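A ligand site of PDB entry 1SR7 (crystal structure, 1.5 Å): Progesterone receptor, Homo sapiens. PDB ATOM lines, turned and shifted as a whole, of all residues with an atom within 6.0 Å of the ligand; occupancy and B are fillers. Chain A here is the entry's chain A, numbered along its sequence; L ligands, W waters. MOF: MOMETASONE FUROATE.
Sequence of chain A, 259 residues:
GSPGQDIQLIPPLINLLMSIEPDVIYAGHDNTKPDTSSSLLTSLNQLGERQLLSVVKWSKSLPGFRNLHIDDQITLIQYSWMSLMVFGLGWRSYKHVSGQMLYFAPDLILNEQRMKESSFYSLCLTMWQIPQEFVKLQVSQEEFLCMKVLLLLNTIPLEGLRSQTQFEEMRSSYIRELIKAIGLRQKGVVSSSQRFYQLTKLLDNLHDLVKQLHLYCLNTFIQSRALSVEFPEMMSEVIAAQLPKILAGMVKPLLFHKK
O35 of the ligand lies within hydrogen-bond range of NH1 of Arg 92, at 2.9 Å.
An oxygen (O21) of the ligand lies within hydrogen-bond range of the side-chain amide oxygen (OD1) of Asn 45, at 3.1 Å.
O35 of the ligand lies close to OE1 of Gln 51 (3.1 Å).
The side-chain amide nitrogen of Gln 51 sits close to the side-chain sulfur of Met 85.
SG of Cys 124 sits at hydrogen-bond distance from O of Phe 120 (3.4 Å).
The side-chain hydroxyl of Thr 220 sits at hydrogen-bond distance from the backbone carbonyl oxygen of Tyr 216, 3.0 Å away.
The backbone carbonyl oxygen of Tyr 103 lies within hydrogen-bond range of the guanidinium group of Arg 92 (3.0 Å).
NH1 of Arg 92 is in hydrogen-bond range of OE1 of Gln 51 (3.4 Å).
The guanidinium group (NH1) of Arg 92 is in hydrogen-bond range of the backbone carbonyl oxygen (O) of Phe 104 (3.0 Å).
CD2 of Leu 41 touches O17 of the ligand, at 3.5 Å.
Leu 44 touches the ligand.
Leu 47 touches the ligand (CD2 to C33, 3.6 Å).
CA of Gly 48 touches C30 of the ligand, 3.7 Å away.
Met 82 touches the ligand (SD to C9, 3.9 Å).
Met 85 touches the ligand.
Val 86 touches the ligand (N to C26, 3.7 Å).
Phe 104 touches the ligand.
Phe 120 touches the ligand (O to C28, 3.6 Å).
CD1 of Leu 123 touches O23 of the ligand (3.6 Å).
Cys 124 touches the ligand.
CE of Met 127 touches C27 of the ligand (3.7 Å).
Leu 213 touches the ligand.
CE2 of Tyr 216 touches O17 of the ligand, 3.1 Å away.
Cys 217 touches the ligand.
CG2 of Thr 220 touches CL18 of the ligand, 3.6 Å away.
CG1 of Val 229 touches CL18 of the ligand, at 3.99 Å.
Phe 231 touches the ligand (CZ to CL18, 3.7 Å).
CE of Met 235 touches O21 of the ligand, 3.4 Å away.
Of the 32 residues printed, 22 come within 4 Å of the ligand.
Water W1 lies within hydrogen-bond range of the side-chain amide nitrogen of Gln 51 (2.7 Å), the backbone carbonyl oxygen of Met 85 (2.7 Å), the guanidinium group of Arg 92 (2.9 Å) and an oxygen (O35) of the ligand (3.4 Å).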
ATOM      1  N   LEU A  41      -6.411 -13.451  -0.241  1.00  0.00           N
ATOM      2  CA  LEU A  41      -6.984 -13.901  -1.499  1.00  0.00           C
ATOM      3  C   LEU A  41      -8.409 -13.469  -1.602  1.00  0.00           C
ATOM      4  O   LEU A  41      -8.874 -13.027  -2.705  1.00  0.00           O
ATOM      5  CB  LEU A  41      -6.916 -15.434  -1.646  1.00  0.00           C
ATOM      6  CG  LEU A  41      -5.521 -15.996  -1.712  1.00  0.00           C
ATOM      7  CD1 LEU A  41      -5.442 -17.571  -1.642  1.00  0.00           C
ATOM      8  CD2 LEU A  41      -4.765 -15.464  -3.022  1.00  0.00           C
ATOM      9  N   LEU A  44      -8.389  -9.937  -2.697  1.00  0.00           N
ATOM     10  CA  LEU A  44      -7.973  -9.800  -4.047  1.00  0.00           C
ATOM     11  C   LEU A  44      -9.175 -10.117  -4.991  1.00  0.00           C
ATOM     12  O   LEU A  44      -9.455  -9.354  -5.980  1.00  0.00           O
ATOM     13  CB  LEU A  44      -6.785 -10.658  -4.384  1.00  0.00           C
ATOM     14  CG  LEU A  44      -5.444 -10.138  -3.724  1.00  0.00           C
ATOM     15  CD1 LEU A  44      -4.477 -11.219  -3.760  1.00  0.00           C
ATOM     16  CD2 LEU A  44      -4.973  -8.812  -4.438  1.00  0.00           C
ATOM     17  N   ASN A  45      -9.950 -11.125  -4.586  1.00  0.00           N
ATOM     18  CA  ASN A  45     -11.119 -11.452  -5.502  1.00  0.00           C
ATOM     19  C   ASN A  45     -12.228 -10.429  -5.373  1.00  0.00           C
ATOM     20  O   ASN A  45     -12.929 -10.163  -6.362  1.00  0.00           O
ATOM     21  CB  ASN A  45     -11.641 -12.813  -5.097  1.00  0.00           C
ATOM     22  CG  ASN A  45     -10.826 -13.908  -5.578  1.00  0.00           C
ATOM     23  OD1 ASN A  45     -10.018 -13.825  -6.500  1.00  0.00           O
ATOM     24  ND2 ASN A  45     -11.063 -15.059  -4.955  1.00  0.00           N
ATOM     25  N   LEU A  47     -11.610  -7.196  -4.870  1.00  0.00           N
ATOM     26  CA  LEU A  47     -11.164  -6.163  -5.750  1.00  0.00           C
ATOM     27  C   LEU A  47     -11.458  -6.557  -7.215  1.00  0.00           C
ATOM     28  O   LEU A  47     -11.855  -5.639  -8.002  1.00  0.00           O
ATOM     29  CB  LEU A  47      -9.598  -5.956  -5.494  1.00  0.00           C
ATOM     30  CG  LEU A  47      -8.972  -4.919  -6.417  1.00  0.00           C
ATOM     31  CD1 LEU A  47      -9.594  -3.565  -6.239  1.00  0.00           C
ATOM     32  CD2 LEU A  47      -7.425  -4.917  -6.021  1.00  0.00           C
ATOM     33  N   GLY A  48     -11.147  -7.812  -7.597  1.00  0.00           N
ATOM     34  CA  GLY A  48     -11.322  -8.333  -8.978  1.00  0.00           C
ATOM     35  C   GLY A  48     -12.824  -8.103  -9.395  1.00  0.00           C
ATOM     36  O   GLY A  48     -13.075  -7.642 -10.515  1.00  0.00           O
ATOM     37  N   GLN A  51     -13.190  -4.516 -10.253  1.00  0.00           N
ATOM     38  CA  GLN A  51     -12.463  -4.228 -11.465  1.00  0.00           C
ATOM     39  C   GLN A  51     -13.218  -4.793 -12.642  1.00  0.00           C
ATOM     40  O   GLN A  51     -13.201  -4.122 -13.663  1.00  0.00           O
ATOM     41  CB  GLN A  51     -10.973  -4.717 -11.418  1.00  0.00           C
ATOM     42  CG  GLN A  51     -10.184  -3.965 -10.358  1.00  0.00           C
ATOM     43  CD  GLN A  51      -8.823  -4.418 -10.358  1.00  0.00           C
ATOM     44  OE1 GLN A  51      -8.004  -3.777  -9.559  1.00  0.00           O
ATOM     45  NE2 GLN A  51      -8.422  -5.374 -11.208  1.00  0.00           N
ATOM     46  N   TRP A  81     -10.454 -10.918 -19.416  1.00  0.00           N
ATOM     47  CA  TRP A  81     -10.558 -10.178 -18.133  1.00  0.00           C
ATOM     48  C   TRP A  81      -9.248 -10.320 -17.328  1.00  0.00           C
ATOM     49  O   TRP A  81      -8.821  -9.290 -16.807  1.00  0.00           O
ATOM     50  CB  TRP A  81     -11.804 -10.555 -17.329  1.00  0.00           C
ATOM     51  CG  TRP A  81     -11.760 -11.987 -16.830  1.00  0.00           C
ATOM     52  CD1 TRP A  81     -12.204 -13.121 -17.528  1.00  0.00           C
ATOM     53  CD2 TRP A  81     -11.363 -12.438 -15.529  1.00  0.00           C
ATOM     54  NE1 TRP A  81     -11.967 -14.249 -16.757  1.00  0.00           N
ATOM     55  CE2 TRP A  81     -11.482 -13.842 -15.520  1.00  0.00           C
ATOM     56  CE3 TRP A  81     -10.863 -11.775 -14.400  1.00  0.00           C
ATOM     57  CZ2 TRP A  81     -11.165 -14.626 -14.419  1.00  0.00           C
ATOM     58  CZ3 TRP A  81     -10.505 -12.588 -13.272  1.00  0.00           C
ATOM     59  CH2 TRP A  81     -10.675 -13.961 -13.304  1.00  0.00           C
ATOM     60  N   MET A  82      -8.747 -11.530 -17.085  1.00  0.00           N
ATOM     61  CA  MET A  82      -7.631 -11.628 -16.124  1.00  0.00           C
ATOM     62  C   MET A  82      -6.438 -11.014 -16.811  1.00  0.00           C
ATOM     63  O   MET A  82      -5.658 -10.318 -16.060  1.00  0.00           O
ATOM     64  CB  MET A  82      -7.350 -13.104 -15.768  1.00  0.00           C
ATOM     65  CG  MET A  82      -6.466 -13.165 -14.204  1.00  0.00           C
ATOM     66  SD  MET A  82      -6.056 -14.778 -14.111  1.00  0.00           S
ATOM     67  CE  MET A  82      -7.525 -15.455 -13.533  1.00  0.00           C
ATOM     68  N   MET A  85      -6.638  -7.342 -16.293  1.00  0.00           N
ATOM     69  CA  MET A  85      -6.474  -6.912 -14.876  1.00  0.00           C
ATOM     70  C   MET A  85      -5.013  -7.077 -14.445  1.00  0.00           C
ATOM     71  O   MET A  85      -4.514  -6.206 -13.716  1.00  0.00           O
ATOM     72  CB  MET A  85      -7.476  -7.653 -13.978  1.00  0.00           C
ATOM     73  CG  MET A  85      -8.908  -6.964 -14.197  1.00  0.00           C
ATOM     74  SD  MET A  85     -10.035  -8.073 -13.235  1.00  0.00           S
ATOM     75  CE  MET A  85     -11.582  -7.896 -14.191  1.00  0.00           C
ATOM     76  N   VAL A  86      -4.337  -8.074 -14.855  1.00  0.00           N
ATOM     77  CA  VAL A  86      -2.882  -8.162 -14.540  1.00  0.00           C
ATOM     78  C   VAL A  86      -2.111  -7.127 -15.323  1.00  0.00           C
ATOM     79  O   VAL A  86      -1.138  -6.583 -14.773  1.00  0.00           O
ATOM     80  CB  VAL A  86      -2.400  -9.582 -14.770  1.00  0.00           C
ATOM     81  CG1 VAL A  86      -2.168  -9.909 -16.125  1.00  0.00           C
ATOM     82  CG2 VAL A  86      -1.024  -9.802 -13.955  1.00  0.00           C
ATOM     83  N   LEU A  89      -2.645  -3.977 -13.316  1.00  0.00           N
ATOM     84  CA  LEU A  89      -1.838  -4.146 -12.049  1.00  0.00           C
ATOM     85  C   LEU A  89      -0.404  -3.781 -12.432  1.00  0.00           C
ATOM     86  O   LEU A  89       0.275  -3.015 -11.643  1.00  0.00           O
ATOM     87  CB  LEU A  89      -1.818  -5.623 -11.550  1.00  0.00           C
ATOM     88  CG  LEU A  89      -0.823  -5.916 -10.452  1.00  0.00           C
ATOM     89  CD1 LEU A  89      -1.054  -5.172  -9.144  1.00  0.00           C
ATOM     90  CD2 LEU A  89      -0.924  -7.444 -10.268  1.00  0.00           C
ATOM     91  N   ARG A  92      -0.168   0.129 -12.708  1.00  0.00           N
ATOM     92  CA  ARG A  92      -0.239   0.849 -11.439  1.00  0.00           C
ATOM     93  C   ARG A  92       1.079   0.631 -10.690  1.00  0.00           C
ATOM     94  O   ARG A  92       1.514   1.529  -9.982  1.00  0.00           O
ATOM     95  CB  ARG A  92      -1.423   0.373 -10.616  1.00  0.00           C
ATOM     96  CG  ARG A  92      -2.748   0.760 -11.294  1.00  0.00           C
ATOM     97  CD  ARG A  92      -3.880   0.458 -10.280  1.00  0.00           C
ATOM     98  NE  ARG A  92      -4.012  -0.967  -9.957  1.00  0.00           N
ATOM     99  CZ  ARG A  92      -4.614  -1.902 -10.692  1.00  0.00           C
ATOM    100  NH1 ARG A  92      -4.749  -3.150 -10.265  1.00  0.00           N
ATOM    101  NH2 ARG A  92      -5.237  -1.518 -11.821  1.00  0.00           N
ATOM    102  N   TYR A 103       0.867  -2.978  -6.735  1.00  0.00           N
ATOM    103  CA  TYR A 103      -0.087  -1.976  -6.397  1.00  0.00           C
ATOM    104  C   TYR A 103      -1.487  -2.450  -6.936  1.00  0.00           C
ATOM    105  O   TYR A 103      -1.952  -2.025  -7.986  1.00  0.00           O
ATOM    106  CB  TYR A 103       0.313  -0.643  -7.012  1.00  0.00           C
ATOM    107  CG  TYR A 103      -0.398   0.537  -6.444  1.00  0.00           C
ATOM    108  CD1 TYR A 103      -1.739   0.862  -6.814  1.00  0.00           C
ATOM    109  CD2 TYR A 103       0.279   1.387  -5.589  1.00  0.00           C
ATOM    110  CE1 TYR A 103      -2.391   2.052  -6.310  1.00  0.00           C
ATOM    111  CE2 TYR A 103      -0.351   2.543  -5.051  1.00  0.00           C
ATOM    112  CZ  TYR A 103      -1.599   2.921  -5.472  1.00  0.00           C
ATOM    113  OH  TYR A 103      -2.269   4.063  -4.998  1.00  0.00           O
ATOM    114  N   PHE A 104      -2.061  -3.327  -6.168  1.00  0.00           N
ATOM    115  CA  PHE A 104      -3.389  -3.879  -6.593  1.00  0.00           C
ATOM    116  C   PHE A 104      -4.418  -2.763  -6.455  1.00  0.00           C
ATOM    117  O   PHE A 104      -5.301  -2.607  -7.376  1.00  0.00           O
ATOM    118  CB  PHE A 104      -3.831  -5.135  -5.751  1.00  0.00           C
ATOM    119  CG  PHE A 104      -3.027  -6.335  -5.983  1.00  0.00           C
ATOM    120  CD1 PHE A 104      -1.846  -6.532  -5.174  1.00  0.00           C
ATOM    121  CD2 PHE A 104      -3.323  -7.216  -7.029  1.00  0.00           C
ATOM    122  CE1 PHE A 104      -1.112  -7.608  -5.290  1.00  0.00           C
ATOM    123  CE2 PHE A 104      -2.451  -8.338  -7.273  1.00  0.00           C
ATOM    124  CZ  PHE A 104      -1.316  -8.500  -6.414  1.00  0.00           C
ATOM    125  N   ALA A 105      -4.360  -1.954  -5.365  1.00  0.00           N
ATOM    126  CA  ALA A 105      -5.295  -0.826  -5.156  1.00  0.00           C
ATOM    127  C   ALA A 105      -4.610   0.075  -4.128  1.00  0.00           C
ATOM    128  O   ALA A 105      -3.642  -0.395  -3.543  1.00  0.00           O
ATOM    129  CB  ALA A 105      -6.624  -1.428  -4.554  1.00  0.00           C
ATOM    130  N   LEU A 110       1.023  -4.752  -1.983  1.00  0.00           N
ATOM    131  CA  LEU A 110       1.838  -5.886  -1.396  1.00  0.00           C
ATOM    132  C   LEU A 110       3.318  -5.701  -1.638  1.00  0.00           C
ATOM    133  O   LEU A 110       3.752  -5.502  -2.759  1.00  0.00           O
ATOM    134  CB  LEU A 110       1.372  -7.208  -1.835  1.00  0.00           C
ATOM    135  CG  LEU A 110      -0.139  -7.445  -1.602  1.00  0.00           C
ATOM    136  CD1 LEU A 110      -0.440  -8.900  -2.019  1.00  0.00           C
ATOM    137  CD2 LEU A 110      -0.656  -7.143  -0.262  1.00  0.00           C
ATOM    138  N   SER A 119       3.344 -20.617  -2.494  1.00  0.00           N
ATOM    139  CA  SER A 119       2.587 -20.490  -3.761  1.00  0.00           C
ATOM    140  C   SER A 119       2.054 -19.006  -3.986  1.00  0.00           C
ATOM    141  O   SER A 119       2.193 -18.519  -5.069  1.00  0.00           O
ATOM    142  CB  SER A 119       1.468 -21.498  -3.869  1.00  0.00           C
ATOM    143  OG  SER A 119       0.412 -21.068  -3.072  1.00  0.00           O
ATOM    144  N   PHE A 120       1.633 -18.379  -2.918  1.00  0.00           N
ATOM    145  CA  PHE A 120       1.284 -16.925  -3.035  1.00  0.00           C
ATOM    146  C   PHE A 120       2.472 -16.050  -3.553  1.00  0.00           C
ATOM    147  O   PHE A 120       2.387 -15.242  -4.498  1.00  0.00           O
ATOM    148  CB  PHE A 120       0.851 -16.494  -1.667  1.00  0.00           C
ATOM    149  CG  PHE A 120       0.213 -15.161  -1.622  1.00  0.00           C
ATOM    150  CD1 PHE A 120       0.935 -13.987  -1.695  1.00  0.00           C
ATOM    151  CD2 PHE A 120      -1.124 -15.078  -1.507  1.00  0.00           C
ATOM    152  CE1 PHE A 120       0.283 -12.717  -1.671  1.00  0.00           C
ATOM    153  CE2 PHE A 120      -1.808 -13.809  -1.483  1.00  0.00           C
ATOM    154  CZ  PHE A 120      -1.123 -12.644  -1.507  1.00  0.00           C
ATOM    155  N   TYR A 121       3.716 -16.297  -3.044  1.00  0.00           N
ATOM    156  CA  TYR A 121       4.826 -15.497  -3.475  1.00  0.00           C
ATOM    157  C   TYR A 121       5.202 -15.856  -4.894  1.00  0.00           C
ATOM    158  O   TYR A 121       5.495 -14.989  -5.739  1.00  0.00           O
ATOM    159  CB  TYR A 121       5.976 -15.798  -2.447  1.00  0.00           C
ATOM    160  CG  TYR A 121       7.261 -15.056  -2.772  1.00  0.00           C
ATOM    161  CD1 TYR A 121       7.303 -13.664  -2.904  1.00  0.00           C
ATOM    162  CD2 TYR A 121       8.472 -15.757  -3.056  1.00  0.00           C
ATOM    163  CE1 TYR A 121       8.492 -12.939  -3.196  1.00  0.00           C
ATOM    164  CE2 TYR A 121       9.681 -15.003  -3.353  1.00  0.00           C
ATOM    165  CZ  TYR A 121       9.649 -13.592  -3.404  1.00  0.00           C
ATOM    166  OH  TYR A 121      10.739 -12.754  -3.733  1.00  0.00           O
ATOM    167  N   LEU A 123       3.182 -16.747  -7.248  1.00  0.00           N
ATOM    168  CA  LEU A 123       2.217 -16.125  -8.162  1.00  0.00           C
ATOM    169  C   LEU A 123       2.496 -14.617  -8.301  1.00  0.00           C
ATOM    170  O   LEU A 123       2.379 -14.036  -9.418  1.00  0.00           O
ATOM    171  CB  LEU A 123       0.762 -16.360  -7.637  1.00  0.00           C
ATOM    172  CG  LEU A 123       0.348 -17.837  -7.808  1.00  0.00           C
ATOM    173  CD1 LEU A 123      -0.830 -18.194  -6.841  1.00  0.00           C
ATOM    174  CD2 LEU A 123      -0.088 -18.058  -9.259  1.00  0.00           C
ATOM    175  N   CYS A 124       2.862 -14.001  -7.172  1.00  0.00           N
ATOM    176  CA  CYS A 124       3.255 -12.589  -7.277  1.00  0.00           C
ATOM    177  C   CYS A 124       4.465 -12.377  -8.180  1.00  0.00           C
ATOM    178  O   CYS A 124       4.518 -11.467  -9.010  1.00  0.00           O
ATOM    179  CB  CYS A 124       3.450 -12.073  -5.875  1.00  0.00           C
ATOM    180  SG  CYS A 124       2.056 -11.829  -4.834  1.00  0.00           S
ATOM    181  N   MET A 127       3.355 -12.313 -11.740  1.00  0.00           N
ATOM    182  CA  MET A 127       2.670 -11.029 -12.076  1.00  0.00           C
ATOM    183  C   MET A 127       3.711  -9.866 -12.199  1.00  0.00           C
ATOM    184  O   MET A 127       3.552  -9.013 -13.062  1.00  0.00           O
ATOM    185  CB  MET A 127       1.582 -10.665 -11.078  1.00  0.00           C
ATOM    186  CG  MET A 127       0.515 -11.700 -11.009  1.00  0.00           C
ATOM    187  SD  MET A 127      -0.896 -11.277 -10.086  1.00  0.00           S
ATOM    188  CE  MET A 127      -0.575 -11.263  -8.890  1.00  0.00           C
ATOM    189  N   GLN A 212      -0.562 -19.641 -16.278  1.00  0.00           N
ATOM    190  CA  GLN A 212      -0.297 -20.042 -14.975  1.00  0.00           C
ATOM    191  C   GLN A 212      -1.316 -19.463 -13.957  1.00  0.00           C
ATOM    192  O   GLN A 212      -1.748 -20.149 -13.066  1.00  0.00           O
ATOM    193  CB  GLN A 212       1.099 -19.577 -14.535  1.00  0.00           C
ATOM    194  CG  GLN A 212       2.192 -19.827 -15.525  1.00  0.00           C
ATOM    195  CD  GLN A 212       3.617 -19.308 -14.985  1.00  0.00           C
ATOM    196  OE1 GLN A 212       4.345 -18.646 -15.721  1.00  0.00           O
ATOM    197  NE2 GLN A 212       3.902 -19.545 -13.701  1.00  0.00           N
ATOM    198  N   LEU A 213      -1.785 -18.191 -14.217  1.00  0.00           N
ATOM    199  CA  LEU A 213      -2.675 -17.543 -13.244  1.00  0.00           C
ATOM    200  C   LEU A 213      -4.125 -18.141 -13.437  1.00  0.00           C
ATOM    201  O   LEU A 213      -4.825 -18.357 -12.478  1.00  0.00           O
ATOM    202  CB  LEU A 213      -2.774 -16.013 -13.575  1.00  0.00           C
ATOM    203  CG  LEU A 213      -1.348 -15.371 -13.501  1.00  0.00           C
ATOM    204  CD1 LEU A 213      -1.649 -13.854 -13.687  1.00  0.00           C
ATOM    205  CD2 LEU A 213      -0.683 -15.585 -12.181  1.00  0.00           C
ATOM    206  N   HIS A 214      -4.419 -18.448 -14.701  1.00  0.00           N
ATOM    207  CA  HIS A 214      -5.728 -19.081 -15.004  1.00  0.00           C
ATOM    208  C   HIS A 214      -5.799 -20.427 -14.342  1.00  0.00           C
ATOM    209  O   HIS A 214      -6.845 -20.733 -13.777  1.00  0.00           O
ATOM    210  CB  HIS A 214      -5.897 -19.312 -16.534  1.00  0.00           C
ATOM    211  CG  HIS A 214      -6.275 -18.075 -17.342  1.00  0.00           C
ATOM    212  ND1 HIS A 214      -6.199 -18.114 -18.705  1.00  0.00           N
ATOM    213  CD2 HIS A 214      -6.877 -16.917 -17.013  1.00  0.00           C
ATOM    214  CE1 HIS A 214      -6.670 -16.990 -19.207  1.00  0.00           C
ATOM    215  NE2 HIS A 214      -7.093 -16.239 -18.194  1.00  0.00           N
ATOM    216  N   TYR A 216      -4.078 -21.556 -11.618  1.00  0.00           N
ATOM    217  CA  TYR A 216      -4.269 -21.429 -10.173  1.00  0.00           C
ATOM    218  C   TYR A 216      -5.626 -20.938  -9.765  1.00  0.00           C
ATOM    219  O   TYR A 216      -6.246 -21.481  -8.840  1.00  0.00           O
ATOM    220  CB  TYR A 216      -3.148 -20.573  -9.609  1.00  0.00           C
ATOM    221  CG  TYR A 216      -3.175 -20.561  -8.047  1.00  0.00           C
ATOM    222  CD1 TYR A 216      -2.372 -21.542  -7.371  1.00  0.00           C
ATOM    223  CD2 TYR A 216      -3.918 -19.647  -7.291  1.00  0.00           C
ATOM    224  CE1 TYR A 216      -2.365 -21.556  -6.049  1.00  0.00           C
ATOM    225  CE2 TYR A 216      -3.897 -19.672  -5.868  1.00  0.00           C
ATOM    226  CZ  TYR A 216      -3.138 -20.630  -5.274  1.00  0.00           C
ATOM    227  OH  TYR A 216      -3.034 -20.708  -3.892  1.00  0.00           O
ATOM    228  N   CYS A 217      -6.164 -19.954 -10.537  1.00  0.00           N
ATOM    229  CA  CYS A 217      -7.507 -19.496 -10.282  1.00  0.00           C
ATOM    230  C   CYS A 217      -8.567 -20.584 -10.335  1.00  0.00           C
ATOM    231  O   CYS A 217      -9.336 -20.744  -9.446  1.00  0.00           O
ATOM    232  CB  CYS A 217      -7.803 -18.334 -11.212  1.00  0.00           C
ATOM    233  SG  CYS A 217      -9.450 -17.699 -11.135  1.00  0.00           S
ATOM    234  N   LEU A 218      -8.488 -21.396 -11.367  1.00  0.00           N
ATOM    235  CA  LEU A 218      -9.584 -22.407 -11.558  1.00  0.00           C
ATOM    236  C   LEU A 218      -9.378 -23.511 -10.489  1.00  0.00           C
ATOM    237  O   LEU A 218     -10.412 -23.915  -9.933  1.00  0.00           O
ATOM    238  CB  LEU A 218      -9.464 -22.983 -12.988  1.00  0.00           C
ATOM    239  CG  LEU A 218     -10.579 -24.042 -13.210  1.00  0.00           C
ATOM    240  CD1 LEU A 218     -11.918 -23.305 -13.145  1.00  0.00           C
ATOM    241  CD2 LEU A 218     -10.350 -24.589 -14.721  1.00  0.00           C
ATOM    242  N   THR A 220      -8.242 -23.140  -7.433  1.00  0.00           N
ATOM    243  CA  THR A 220      -8.728 -22.592  -6.122  1.00  0.00           C
ATOM    244  C   THR A 220     -10.252 -22.583  -6.254  1.00  0.00           C
ATOM    245  O   THR A 220     -11.006 -22.944  -5.328  1.00  0.00           O
ATOM    246  CB  THR A 220      -8.171 -21.233  -5.909  1.00  0.00           C
ATOM    247  OG1 THR A 220      -6.769 -21.308  -5.881  1.00  0.00           O
ATOM    248  CG2 THR A 220      -8.653 -20.591  -4.605  1.00  0.00           C
ATOM    249  N   VAL A 229     -11.925 -19.513   0.517  1.00  0.00           N
ATOM    250  CA  VAL A 229     -11.585 -18.415  -0.437  1.00  0.00           C
ATOM    251  C   VAL A 229     -12.890 -18.084  -1.164  1.00  0.00           C
ATOM    252  O   VAL A 229     -13.373 -18.901  -1.934  1.00  0.00           O
ATOM    253  CB  VAL A 229     -10.453 -18.682  -1.418  1.00  0.00           C
ATOM    254  CG1 VAL A 229     -10.297 -17.460  -2.465  1.00  0.00           C
ATOM    255  CG2 VAL A 229      -9.006 -18.910  -0.770  1.00  0.00           C
ATOM    256  N   PHE A 231     -15.141 -16.299  -4.010  1.00  0.00           N
ATOM    257  CA  PHE A 231     -15.160 -15.681  -5.317  1.00  0.00           C
ATOM    258  C   PHE A 231     -16.493 -15.051  -5.511  1.00  0.00           C
ATOM    259  O   PHE A 231     -17.513 -15.748  -5.404  1.00  0.00           O
ATOM    260  CB  PHE A 231     -15.048 -16.738  -6.378  1.00  0.00           C
ATOM    261  CG  PHE A 231     -13.593 -17.304  -6.469  1.00  0.00           C
ATOM    262  CD1 PHE A 231     -13.142 -18.279  -5.581  1.00  0.00           C
ATOM    263  CD2 PHE A 231     -12.742 -16.864  -7.466  1.00  0.00           C
ATOM    264  CE1 PHE A 231     -11.873 -18.749  -5.661  1.00  0.00           C
ATOM    265  CE2 PHE A 231     -11.428 -17.346  -7.595  1.00  0.00           C
ATOM    266  CZ  PHE A 231     -10.992 -18.302  -6.663  1.00  0.00           C
ATOM    267  N   MET A 235     -17.439 -12.519 -10.961  1.00  0.00           N
ATOM    268  CA  MET A 235     -16.180 -13.215 -11.288  1.00  0.00           C
ATOM    269  C   MET A 235     -16.446 -14.733 -11.369  1.00  0.00           C
ATOM    270  O   MET A 235     -15.860 -15.377 -12.227  1.00  0.00           O
ATOM    271  CB  MET A 235     -15.179 -13.007 -10.135  1.00  0.00           C
ATOM    272  CG  MET A 235     -13.800 -13.589 -10.655  1.00  0.00           C
ATOM    273  SD  MET A 235     -12.598 -13.337  -9.271  1.00  0.00           S
ATOM    274  CE  MET A 235     -11.259 -13.745 -10.121  1.00  0.00           C
HETATM  275  O35 MOF L   1      -5.677  -5.783  -9.388  1.00  0.00           O
HETATM  276  C34 MOF L   1      -6.138  -6.896  -9.564  1.00  0.00           C
HETATM  277  C33 MOF L   1      -7.186  -7.392  -8.629  1.00  0.00           C
HETATM  278  C32 MOF L   1      -5.557  -7.813 -10.566  1.00  0.00           C
HETATM  279  C29 MOF L   1      -5.929  -9.140 -10.709  1.00  0.00           C
HETATM  280  C26 MOF L   1      -5.264 -10.023 -11.789  1.00  0.00           C
HETATM  281  C24 MOF L   1      -7.078  -9.717  -9.898  1.00  0.00           C
HETATM  282  C30 MOF L   1      -7.629  -8.795  -8.820  1.00  0.00           C
HETATM  283  C31 MOF L   1      -8.265  -9.936 -10.868  1.00  0.00           C
HETATM  284  C19 MOF L   1      -6.531 -11.033  -9.273  1.00  0.00           C
HETATM  285 CL25 MOF L   1      -5.103 -10.600  -8.180  1.00  0.00          CL
HETATM  286  C15 MOF L   1      -7.490 -11.729  -8.279  1.00  0.00           C
HETATM  287  O21 MOF L   1      -8.822 -11.930  -8.654  1.00  0.00           O
HETATM  288  C14 MOF L   1      -5.987 -12.017 -10.349  1.00  0.00           C
HETATM  289  C20 MOF L   1      -4.846 -11.343 -11.091  1.00  0.00           C
HETATM  290  C6  MOF L   1      -5.581 -13.324  -9.684  1.00  0.00           C
HETATM  291  C9  MOF L   1      -4.853 -14.483 -10.439  1.00  0.00           C
HETATM  292  C3  MOF L   1      -4.880 -15.601  -9.463  1.00  0.00           C
HETATM  293  C10 MOF L   1      -3.519 -16.304  -9.479  1.00  0.00           C
HETATM  294  C2  MOF L   1      -6.521 -13.971  -8.659  1.00  0.00           C
HETATM  295  C7  MOF L   1      -6.956 -12.911  -7.580  1.00  0.00           C
HETATM  296  C8  MOF L   1      -7.802 -14.420  -9.422  1.00  0.00           C
HETATM  297  C1  MOF L   1      -5.688 -15.199  -8.229  1.00  0.00           C
HETATM  298  C5  MOF L   1      -6.475 -16.179  -7.509  1.00  0.00           C
HETATM  299  O13 MOF L   1      -6.634 -17.288  -8.043  1.00  0.00           O
HETATM  300  C12 MOF L   1      -7.136 -15.786  -6.280  1.00  0.00           C
HETATM  301 CL18 MOF L   1      -7.631 -17.206  -5.417  1.00  0.00          CL
HETATM  302  O4  MOF L   1      -4.699 -14.546  -7.345  1.00  0.00           O
HETATM  303  C11 MOF L   1      -4.003 -15.388  -6.503  1.00  0.00           C
HETATM  304  O17 MOF L   1      -4.220 -16.576  -6.302  1.00  0.00           O
HETATM  305  C16 MOF L   1      -2.850 -14.637  -5.996  1.00  0.00           C
HETATM  306  C22 MOF L   1      -2.603 -13.392  -6.350  1.00  0.00           C
HETATM  307  C27 MOF L   1      -1.426 -12.996  -5.701  1.00  0.00           C
HETATM  308  C28 MOF L   1      -0.969 -14.109  -4.978  1.00  0.00           C
HETATM  309  O23 MOF L   1      -1.860 -15.167  -5.149  1.00  0.00           O
HETATM  310  O   HOH W   1      -6.205  -4.453 -12.468  1.00  0.00           O
